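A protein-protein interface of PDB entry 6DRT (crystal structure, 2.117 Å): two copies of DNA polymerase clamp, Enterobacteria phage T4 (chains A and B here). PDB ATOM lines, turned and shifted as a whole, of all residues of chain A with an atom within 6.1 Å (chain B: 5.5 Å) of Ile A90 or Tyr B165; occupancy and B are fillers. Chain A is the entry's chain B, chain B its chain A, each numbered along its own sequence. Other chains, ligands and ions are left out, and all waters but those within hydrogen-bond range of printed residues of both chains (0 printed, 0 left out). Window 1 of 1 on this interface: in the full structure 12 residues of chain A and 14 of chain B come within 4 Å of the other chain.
The backbone carbonyl oxygen (O) of Gly B151 lies within hydrogen-bond range of the backbone NH (N) of Lys B164 (3.0 Å).
The backbone carbonyl oxygen (O) of Ile A90 lies within hydrogen-bond range of the backbone NH (N) of Ile A83 (2.7 Å).
O of Tyr B165 sits at hydrogen-bond distance from N of Gly B151, at 2.7 Å.
The backbone carbonyl oxygen of Leu B133 is in hydrogen-bond range of the side-chain amino group of Lys B164.
The side-chain amide oxygen (OE1) of Gln B125 is in hydrogen-bond range of the side-chain hydroxyl (OH) of Tyr B165, 2.8 Å away.
O of Ile A81 sits at hydrogen-bond distance from N of Trp A92 (2.9 Å).
Of the 14 printed residues of chain B, 7 touch a printed residue of chain A.
Hydrophobic or aromatic side chains of chain B that line the printed part of chain A: Val B129, Leu B133 and Tyr B165.
Of the 13 printed residues of chain A, 9 touch a printed residue of chain B.
Printed residues of chain A that touch a printed residue of chain B: Ile A63, Leu A66, Val A67, Asp A85, Ser A88, Thr A89, Ile A90, Phe A91 and Trp A92.
Hydrophobic or aromatic side chains of chain A that line the printed part of chain B: Ile A63, Leu A66, Val A67, Ile A90, Phe A91 and Trp A92.
Along chain A the printed residues that touch a printed residue of chain B span positions 63 to 92.
Among the printed residues, 18 pairs touch across the chains.
Among the printed residues, no Asp or Glu carboxylate lies within 4 Å of a Lys or Arg side-chain nitrogen of the other chain.
N of Phe A91 lies within hydrogen-bond range of O of Lys B164, 2.9 Å away.
N of Thr A89 sits at hydrogen-bond distance from O of Ser B166, 2.9 Å away.
The side-chain amide nitrogen of Gln B125 sits at hydrogen-bond distance from the side-chain carboxylate of Asp A85 (3.0 Å).
O of Leu A66 is in hydrogen-bond range of NE2 of Gln B125 (2.7 Å).
The side-chain amide oxygen (OE1) of Gln B125 lies within hydrogen-bond range of the side-chain hydroxyl (OG) of Ser A88 (2.6 Å).
Ile A63 touches Leu B133.
CG1 of Val A67 touches NE2 of Gln B125, at 3.8 Å.
Tyr B165 touches Ser A88 (OH to CB, 3.7 Å).
O of Ser B166 touches CA of Ser A88 (3.1 Å).
Tyr B165 touches Thr A89 (CA to O, 3.4 Å).
Val B129 touches Ile A90 (CG2 to CD1, 3.8 Å).
Lys B164 touches Ile A90.
Phe A91 touches Leu B133 (O to CD2, 3.7 Å).
Phe A91 touches Val B163 (CD2 to O, 3.3 Å).
Trp A92 touches Leu B133 (CE3 to CD2, 3.8 Å).
No position is printed for both chains.
Of the 18 pairs that touch across the chains among the printed residues, none has its exchanged pair printed and touching as well.
Of chain B, only Val B129, Leu B133, Lys B164 and Tyr B165 come within 4 Å of Ile A90.
Tyr B165 touches three residues of chain A.
Of the printed residues of chain B, Leu A66 touches Gln B125 and Val B129.
Printed residues of chain B within 4 Å of Phe A91: Leu B133, Val B163 and Lys B164.
Of the printed residues of chain A, Gln B125 touches Leu A66 (2.7 Å), Val A67 (3.8 Å), Asp A85 (3.0 Å) and Ser A88 (2.6 Å).
Leu B167 touches none of the printed residues of chain A.
The nearest residue of chain B that does not touch Ile A90 is Gln B125 (5.2 Å).
The nearest residue of chain A that does not touch Tyr B165 is Phe A91 (4.5 Å).
The nearest printed residue of chain B that does not touch Trp A92 is Lys B164 (5.4 Å).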
ATOM      1  N   ILE A  63      25.624   7.541 -13.056  1.00  0.00           N
ATOM      2  CA  ILE A  63      24.937   7.992 -14.260  1.00  0.00           C
ATOM      3  C   ILE A  63      24.951   9.512 -14.356  1.00  0.00           C
ATOM      4  O   ILE A  63      25.007  10.070 -15.460  1.00  0.00           O
ATOM      5  CB  ILE A  63      23.508   7.421 -14.291  1.00  0.00           C
ATOM      6  CG1 ILE A  63      23.406   6.338 -15.363  1.00  0.00           C
ATOM      7  CG2 ILE A  63      22.471   8.514 -14.517  1.00  0.00           C
ATOM      8  CD1 ILE A  63      22.007   5.869 -15.597  1.00  0.00           C
ATOM      9  N   LEU A  66      27.701  10.905 -16.361  1.00  0.00           N
ATOM     10  CA  LEU A  66      27.660  10.675 -17.798  1.00  0.00           C
ATOM     11  C   LEU A  66      26.826  11.715 -18.537  1.00  0.00           C
ATOM     12  O   LEU A  66      26.632  11.590 -19.751  1.00  0.00           O
ATOM     13  CB  LEU A  66      27.130   9.271 -18.091  1.00  0.00           C
ATOM     14  CG  LEU A  66      27.979   8.129 -17.529  1.00  0.00           C
ATOM     15  CD1 LEU A  66      27.362   6.778 -17.856  1.00  0.00           C
ATOM     16  CD2 LEU A  66      29.402   8.215 -18.057  1.00  0.00           C
ATOM     17  N   VAL A  67      26.332  12.734 -17.836  1.00  0.00           N
ATOM     18  CA  VAL A  67      25.583  13.821 -18.448  1.00  0.00           C
ATOM     19  C   VAL A  67      26.300  15.133 -18.144  1.00  0.00           C
ATOM     20  O   VAL A  67      27.237  15.188 -17.348  1.00  0.00           O
ATOM     21  CB  VAL A  67      24.121  13.873 -17.964  1.00  0.00           C
ATOM     22  CG1 VAL A  67      23.402  12.578 -18.308  1.00  0.00           C
ATOM     23  CG2 VAL A  67      24.066  14.139 -16.469  1.00  0.00           C
ATOM     24  N   ILE A  81      12.509   9.014 -11.880  1.00  0.00           N
ATOM     25  CA  ILE A  81      13.459  10.118 -11.951  1.00  0.00           C
ATOM     26  C   ILE A  81      13.817  10.356 -13.410  1.00  0.00           C
ATOM     27  O   ILE A  81      14.204   9.422 -14.122  1.00  0.00           O
ATOM     28  CB  ILE A  81      14.719   9.835 -11.117  1.00  0.00           C
ATOM     29  CG1 ILE A  81      14.344   9.539  -9.664  1.00  0.00           C
ATOM     30  CG2 ILE A  81      15.686  11.008 -11.196  1.00  0.00           C
ATOM     31  CD1 ILE A  81      15.523   9.152  -8.798  1.00  0.00           C
ATOM     32  N   LYS A  82      13.691  11.605 -13.851  1.00  0.00           N
ATOM     33  CA  LYS A  82      14.027  12.007 -15.209  1.00  0.00           C
ATOM     34  C   LYS A  82      15.273  12.880 -15.181  1.00  0.00           C
ATOM     35  O   LYS A  82      15.320  13.879 -14.457  1.00  0.00           O
ATOM     36  CB  LYS A  82      12.865  12.761 -15.861  1.00  0.00           C
ATOM     37  CG  LYS A  82      13.183  13.329 -17.232  1.00  0.00           C
ATOM     38  CD  LYS A  82      12.009  14.123 -17.782  1.00  0.00           C
ATOM     39  CE  LYS A  82      12.362  14.789 -19.102  1.00  0.00           C
ATOM     40  NZ  LYS A  82      11.228  15.590 -19.641  1.00  0.00           N
ATOM     41  N   ILE A  83      16.276  12.499 -15.966  1.00  0.00           N
ATOM     42  CA  ILE A  83      17.524  13.246 -16.081  1.00  0.00           C
ATOM     43  C   ILE A  83      17.606  13.734 -17.522  1.00  0.00           C
ATOM     44  O   ILE A  83      17.929  12.963 -18.433  1.00  0.00           O
ATOM     45  CB  ILE A  83      18.745  12.401 -15.704  1.00  0.00           C
ATOM     46  CG1 ILE A  83      18.581  11.838 -14.291  1.00  0.00           C
ATOM     47  CG2 ILE A  83      20.018  13.229 -15.807  1.00  0.00           C
ATOM     48  CD1 ILE A  83      19.668  10.865 -13.889  1.00  0.00           C
ATOM     49  N   ALA A  84      17.312  15.014 -17.734  1.00  0.00           N
ATOM     50  CA  ALA A  84      17.250  15.588 -19.072  1.00  0.00           C
ATOM     51  C   ALA A  84      18.598  16.201 -19.432  1.00  0.00           C
ATOM     52  O   ALA A  84      19.081  17.105 -18.742  1.00  0.00           O
ATOM     53  CB  ALA A  84      16.143  16.638 -19.155  1.00  0.00           C
ATOM     54  N   ASP A  85      19.198  15.710 -20.512  1.00  0.00           N
ATOM     55  CA  ASP A  85      20.442  16.245 -21.034  1.00  0.00           C
ATOM     56  C   ASP A  85      20.135  17.118 -22.252  1.00  0.00           C
ATOM     57  O   ASP A  85      18.983  17.476 -22.511  1.00  0.00           O
ATOM     58  CB  ASP A  85      21.404  15.099 -21.363  1.00  0.00           C
ATOM     59  CG  ASP A  85      22.859  15.528 -21.329  1.00  0.00           C
ATOM     60  OD1 ASP A  85      23.128  16.743 -21.434  1.00  0.00           O
ATOM     61  OD2 ASP A  85      23.735  14.646 -21.200  1.00  0.00           O
ATOM     62  N   SER A  88      19.559  14.027 -24.926  1.00  0.00           N
ATOM     63  CA  SER A  88      19.242  12.710 -24.398  1.00  0.00           C
ATOM     64  C   SER A  88      18.481  12.846 -23.088  1.00  0.00           C
ATOM     65  O   SER A  88      18.478  13.902 -22.451  1.00  0.00           O
ATOM     66  CB  SER A  88      20.508  11.867 -24.188  1.00  0.00           C
ATOM     67  OG  SER A  88      21.379  12.479 -23.254  1.00  0.00           O
ATOM     68  N   THR A  89      17.834  11.752 -22.693  1.00  0.00           N
ATOM     69  CA  THR A  89      17.081  11.689 -21.449  1.00  0.00           C
ATOM     70  C   THR A  89      17.329  10.340 -20.795  1.00  0.00           C
ATOM     71  O   THR A  89      17.283   9.305 -21.466  1.00  0.00           O
ATOM     72  CB  THR A  89      15.578  11.888 -21.691  1.00  0.00           C
ATOM     73  OG1 THR A  89      15.358  13.147 -22.340  1.00  0.00           O
ATOM     74  CG2 THR A  89      14.817  11.864 -20.373  1.00  0.00           C
ATOM     75  N   ILE A  90      17.601  10.357 -19.492  1.00  0.00           N
ATOM     76  CA  ILE A  90      17.837   9.150 -18.711  1.00  0.00           C
ATOM     77  C   ILE A  90      16.718   9.013 -17.688  1.00  0.00           C
ATOM     78  O   ILE A  90      16.332   9.994 -17.042  1.00  0.00           O
ATOM     79  CB  ILE A  90      19.215   9.185 -18.019  1.00  0.00           C
ATOM     80  CG1 ILE A  90      20.332   9.252 -19.062  1.00  0.00           C
ATOM     81  CG2 ILE A  90      19.395   7.975 -17.117  1.00  0.00           C
ATOM     82  CD1 ILE A  90      21.721   9.272 -18.467  1.00  0.00           C
ATOM     83  N   PHE A  91      16.193   7.799 -17.549  1.00  0.00           N
ATOM     84  CA  PHE A  91      15.140   7.495 -16.587  1.00  0.00           C
ATOM     85  C   PHE A  91      15.701   6.543 -15.537  1.00  0.00           C
ATOM     86  O   PHE A  91      16.056   5.402 -15.851  1.00  0.00           O
ATOM     87  CB  PHE A  91      13.919   6.895 -17.282  1.00  0.00           C
ATOM     88  CG  PHE A  91      13.249   7.834 -18.244  1.00  0.00           C
ATOM     89  CD1 PHE A  91      12.344   8.781 -17.792  1.00  0.00           C
ATOM     90  CD2 PHE A  91      13.524   7.771 -19.600  1.00  0.00           C
ATOM     91  CE1 PHE A  91      11.725   9.648 -18.675  1.00  0.00           C
ATOM     92  CE2 PHE A  91      12.909   8.636 -20.488  1.00  0.00           C
ATOM     93  CZ  PHE A  91      12.008   9.575 -20.024  1.00  0.00           C
ATOM     94  N   TRP A  92      15.785   7.017 -14.296  1.00  0.00           N
ATOM     95  CA  TRP A  92      16.229   6.190 -13.189  1.00  0.00           C
ATOM     96  C   TRP A  92      15.041   5.804 -12.316  1.00  0.00           C
ATOM     97  O   TRP A  92      14.191   6.651 -12.019  1.00  0.00           O
ATOM     98  CB  TRP A  92      17.276   6.919 -12.338  1.00  0.00           C
ATOM     99  CG  TRP A  92      18.001   6.021 -11.385  1.00  0.00           C
ATOM    100  CD1 TRP A  92      17.713   5.819 -10.067  1.00  0.00           C
ATOM    101  CD2 TRP A  92      19.134   5.193 -11.679  1.00  0.00           C
ATOM    102  NE1 TRP A  92      18.598   4.920  -9.521  1.00  0.00           N
ATOM    103  CE2 TRP A  92      19.480   4.521 -10.491  1.00  0.00           C
ATOM    104  CE3 TRP A  92      19.890   4.958 -12.832  1.00  0.00           C
ATOM    105  CZ2 TRP A  92      20.549   3.630 -10.421  1.00  0.00           C
ATOM    106  CZ3 TRP A  92      20.951   4.070 -12.761  1.00  0.00           C
ATOM    107  CH2 TRP A  92      21.270   3.418 -11.564  1.00  0.00           C
ATOM    108  N   ASP B 122      27.855  11.364 -28.309  1.00  0.00           N
ATOM    109  CA  ASP B 122      26.568  10.710 -28.094  1.00  0.00           C
ATOM    110  C   ASP B 122      26.712   9.193 -28.099  1.00  0.00           C
ATOM    111  O   ASP B 122      26.093   8.502 -27.282  1.00  0.00           O
ATOM    112  CB  ASP B 122      25.564  11.163 -29.154  1.00  0.00           C
ATOM    113  CG  ASP B 122      25.243  12.640 -29.054  1.00  0.00           C
ATOM    114  OD1 ASP B 122      25.430  13.216 -27.962  1.00  0.00           O
ATOM    115  OD2 ASP B 122      24.802  13.227 -30.065  1.00  0.00           O
ATOM    116  N   GLN B 125      28.190   8.313 -24.753  1.00  0.00           N
ATOM    117  CA  GLN B 125      27.208   8.300 -23.674  1.00  0.00           C
ATOM    118  C   GLN B 125      26.316   7.069 -23.756  1.00  0.00           C
ATOM    119  O   GLN B 125      25.995   6.461 -22.728  1.00  0.00           O
ATOM    120  CB  GLN B 125      26.363   9.575 -23.706  1.00  0.00           C
ATOM    121  CG  GLN B 125      25.350   9.659 -22.573  1.00  0.00           C
ATOM    122  CD  GLN B 125      24.509  10.917 -22.623  1.00  0.00           C
ATOM    123  OE1 GLN B 125      23.588  11.032 -23.431  1.00  0.00           O
ATOM    124  NE2 GLN B 125      24.820  11.871 -21.752  1.00  0.00           N
ATOM    125  N   LEU B 126      25.915   6.681 -24.968  1.00  0.00           N
ATOM    126  CA  LEU B 126      25.068   5.504 -25.135  1.00  0.00           C
ATOM    127  C   LEU B 126      25.742   4.254 -24.580  1.00  0.00           C
ATOM    128  O   LEU B 126      25.114   3.459 -23.870  1.00  0.00           O
ATOM    129  CB  LEU B 126      24.724   5.313 -26.612  1.00  0.00           C
ATOM    130  CG  LEU B 126      24.059   3.990 -26.996  1.00  0.00           C
ATOM    131  CD1 LEU B 126      22.711   3.845 -26.309  1.00  0.00           C
ATOM    132  CD2 LEU B 126      23.914   3.879 -28.508  1.00  0.00           C
ATOM    133  N   VAL B 129      26.152   4.697 -20.564  1.00  0.00           N
ATOM    134  CA  VAL B 129      24.888   4.679 -19.832  1.00  0.00           C
ATOM    135  C   VAL B 129      24.265   3.289 -19.868  1.00  0.00           C
ATOM    136  O   VAL B 129      23.630   2.860 -18.896  1.00  0.00           O
ATOM    137  CB  VAL B 129      23.934   5.751 -20.394  1.00  0.00           C
ATOM    138  CG1 VAL B 129      22.524   5.566 -19.855  1.00  0.00           C
ATOM    139  CG2 VAL B 129      24.440   7.143 -20.051  1.00  0.00           C
ATOM    140  N   LEU B 133      22.665   1.422 -16.670  1.00  0.00           N
ATOM    141  CA  LEU B 133      21.224   1.212 -16.722  1.00  0.00           C
ATOM    142  C   LEU B 133      20.841  -0.226 -17.035  1.00  0.00           C
ATOM    143  O   LEU B 133      19.645  -0.528 -17.100  1.00  0.00           O
ATOM    144  CB  LEU B 133      20.587   2.138 -17.763  1.00  0.00           C
ATOM    145  CG  LEU B 133      20.076   3.488 -17.266  1.00  0.00           C
ATOM    146  CD1 LEU B 133      19.453   4.277 -18.405  1.00  0.00           C
ATOM    147  CD2 LEU B 133      19.083   3.307 -16.128  1.00  0.00           C
ATOM    148  N   ILE B 135      21.114  -1.746 -19.866  1.00  0.00           N
ATOM    149  CA  ILE B 135      20.455  -1.724 -21.165  1.00  0.00           C
ATOM    150  C   ILE B 135      21.106  -2.776 -22.053  1.00  0.00           C
ATOM    151  O   ILE B 135      22.300  -2.689 -22.361  1.00  0.00           O
ATOM    152  CB  ILE B 135      20.538  -0.331 -21.807  1.00  0.00           C
ATOM    153  CG1 ILE B 135      19.709   0.672 -21.002  1.00  0.00           C
ATOM    154  CG2 ILE B 135      20.076  -0.380 -23.258  1.00  0.00           C
ATOM    155  CD1 ILE B 135      19.878   2.097 -21.455  1.00  0.00           C
ATOM    156  N   ILE B 149      17.100   6.932 -30.588  1.00  0.00           N
ATOM    157  CA  ILE B 149      17.510   5.625 -30.087  1.00  0.00           C
ATOM    158  C   ILE B 149      16.953   5.482 -28.679  1.00  0.00           C
ATOM    159  O   ILE B 149      17.228   6.317 -27.810  1.00  0.00           O
ATOM    160  CB  ILE B 149      19.038   5.465 -30.094  1.00  0.00           C
ATOM    161  CG1 ILE B 149      19.578   5.529 -31.522  1.00  0.00           C
ATOM    162  CG2 ILE B 149      19.441   4.156 -29.423  1.00  0.00           C
ATOM    163  CD1 ILE B 149      21.084   5.389 -31.613  1.00  0.00           C
ATOM    164  N   ASN B 150      16.164   4.435 -28.457  1.00  0.00           N
ATOM    165  CA  ASN B 150      15.594   4.141 -27.148  1.00  0.00           C
ATOM    166  C   ASN B 150      16.259   2.898 -26.576  1.00  0.00           C
ATOM    167  O   ASN B 150      16.413   1.894 -27.278  1.00  0.00           O
ATOM    168  CB  ASN B 150      14.080   3.936 -27.238  1.00  0.00           C
ATOM    169  CG  ASN B 150      13.339   5.211 -27.578  1.00  0.00           C
ATOM    170  OD1 ASN B 150      13.812   6.313 -27.296  1.00  0.00           O
ATOM    171  ND2 ASN B 150      12.165   5.069 -28.183  1.00  0.00           N
ATOM    172  N   GLY B 151      16.649   2.968 -25.307  1.00  0.00           N
ATOM    173  CA  GLY B 151      17.297   1.857 -24.627  1.00  0.00           C
ATOM    174  C   GLY B 151      16.328   1.138 -23.707  1.00  0.00           C
ATOM    175  O   GLY B 151      15.494   1.765 -23.052  1.00  0.00           O
ATOM    176  N   VAL B 163      11.060   2.805 -21.602  1.00  0.00           N
ATOM    177  CA  VAL B 163      12.260   3.473 -22.093  1.00  0.00           C
ATOM    178  C   VAL B 163      13.113   3.894 -20.904  1.00  0.00           C
ATOM    179  O   VAL B 163      12.669   4.662 -20.042  1.00  0.00           O
ATOM    180  CB  VAL B 163      11.899   4.677 -22.971  1.00  0.00           C
ATOM    181  CG1 VAL B 163      13.162   5.378 -23.454  1.00  0.00           C
ATOM    182  CG2 VAL B 163      11.043   4.239 -24.148  1.00  0.00           C
ATOM    183  N   LYS B 164      14.345   3.389 -20.850  1.00  0.00           N
ATOM    184  CA  LYS B 164      15.289   3.792 -19.818  1.00  0.00           C
ATOM    185  C   LYS B 164      16.251   4.873 -20.286  1.00  0.00           C
ATOM    186  O   LYS B 164      16.772   5.621 -19.451  1.00  0.00           O
ATOM    187  CB  LYS B 164      16.088   2.577 -19.325  1.00  0.00           C
ATOM    188  CG  LYS B 164      15.218   1.387 -18.947  1.00  0.00           C
ATOM    189  CD  LYS B 164      16.024   0.286 -18.280  1.00  0.00           C
ATOM    190  CE  LYS B 164      16.518   0.717 -16.909  1.00  0.00           C
ATOM    191  NZ  LYS B 164      17.237  -0.382 -16.208  1.00  0.00           N
ATOM    192  N   TYR B 165      16.484   4.980 -21.592  1.00  0.00           N
ATOM    193  CA  TYR B 165      17.382   5.977 -22.153  1.00  0.00           C
ATOM    194  C   TYR B 165      16.914   6.309 -23.561  1.00  0.00           C
ATOM    195  O   TYR B 165      16.498   5.420 -24.308  1.00  0.00           O
ATOM    196  CB  TYR B 165      18.830   5.475 -22.166  1.00  0.00           C
ATOM    197  CG  TYR B 165      19.809   6.378 -22.883  1.00  0.00           C
ATOM    198  CD1 TYR B 165      20.286   7.535 -22.282  1.00  0.00           C
ATOM    199  CD2 TYR B 165      20.273   6.061 -24.153  1.00  0.00           C
ATOM    200  CE1 TYR B 165      21.186   8.358 -22.931  1.00  0.00           C
ATOM    201  CE2 TYR B 165      21.174   6.877 -24.809  1.00  0.00           C
ATOM    202  CZ  TYR B 165      21.626   8.024 -24.194  1.00  0.00           C
ATOM    203  OH  TYR B 165      22.524   8.839 -24.845  1.00  0.00           O
ATOM    204  N   SER B 166      16.980   7.589 -23.916  1.00  0.00           N
ATOM    205  CA  SER B 166      16.543   8.047 -25.228  1.00  0.00           C
ATOM    206  C   SER B 166      17.522   9.085 -25.749  1.00  0.00           C
ATOM    207  O   SER B 166      17.801  10.072 -25.064  1.00  0.00           O
ATOM    208  CB  SER B 166      15.129   8.635 -25.167  1.00  0.00           C
ATOM    209  OG  SER B 166      14.705   9.057 -26.450  1.00  0.00           O
ATOM    210  N   LEU B 167      18.035   8.864 -26.958  1.00  0.00           N
ATOM    211  CA  LEU B 167      18.984   9.764 -27.598  1.00  0.00           C
ATOM    212  C   LEU B 167      18.420  10.232 -28.931  1.00  0.00           C
ATOM    213  O   LEU B 167      17.990   9.411 -29.747  1.00  0.00           O
ATOM    214  CB  LEU B 167      20.335   9.075 -27.811  1.00  0.00           C
ATOM    215  CG  LEU B 167      21.330   9.783 -28.734  1.00  0.00           C
ATOM    216  CD1 LEU B 167      21.791  11.101 -28.130  1.00  0.00           C
ATOM    217  CD2 LEU B 167      22.516   8.877 -29.041  1.00  0.00           C
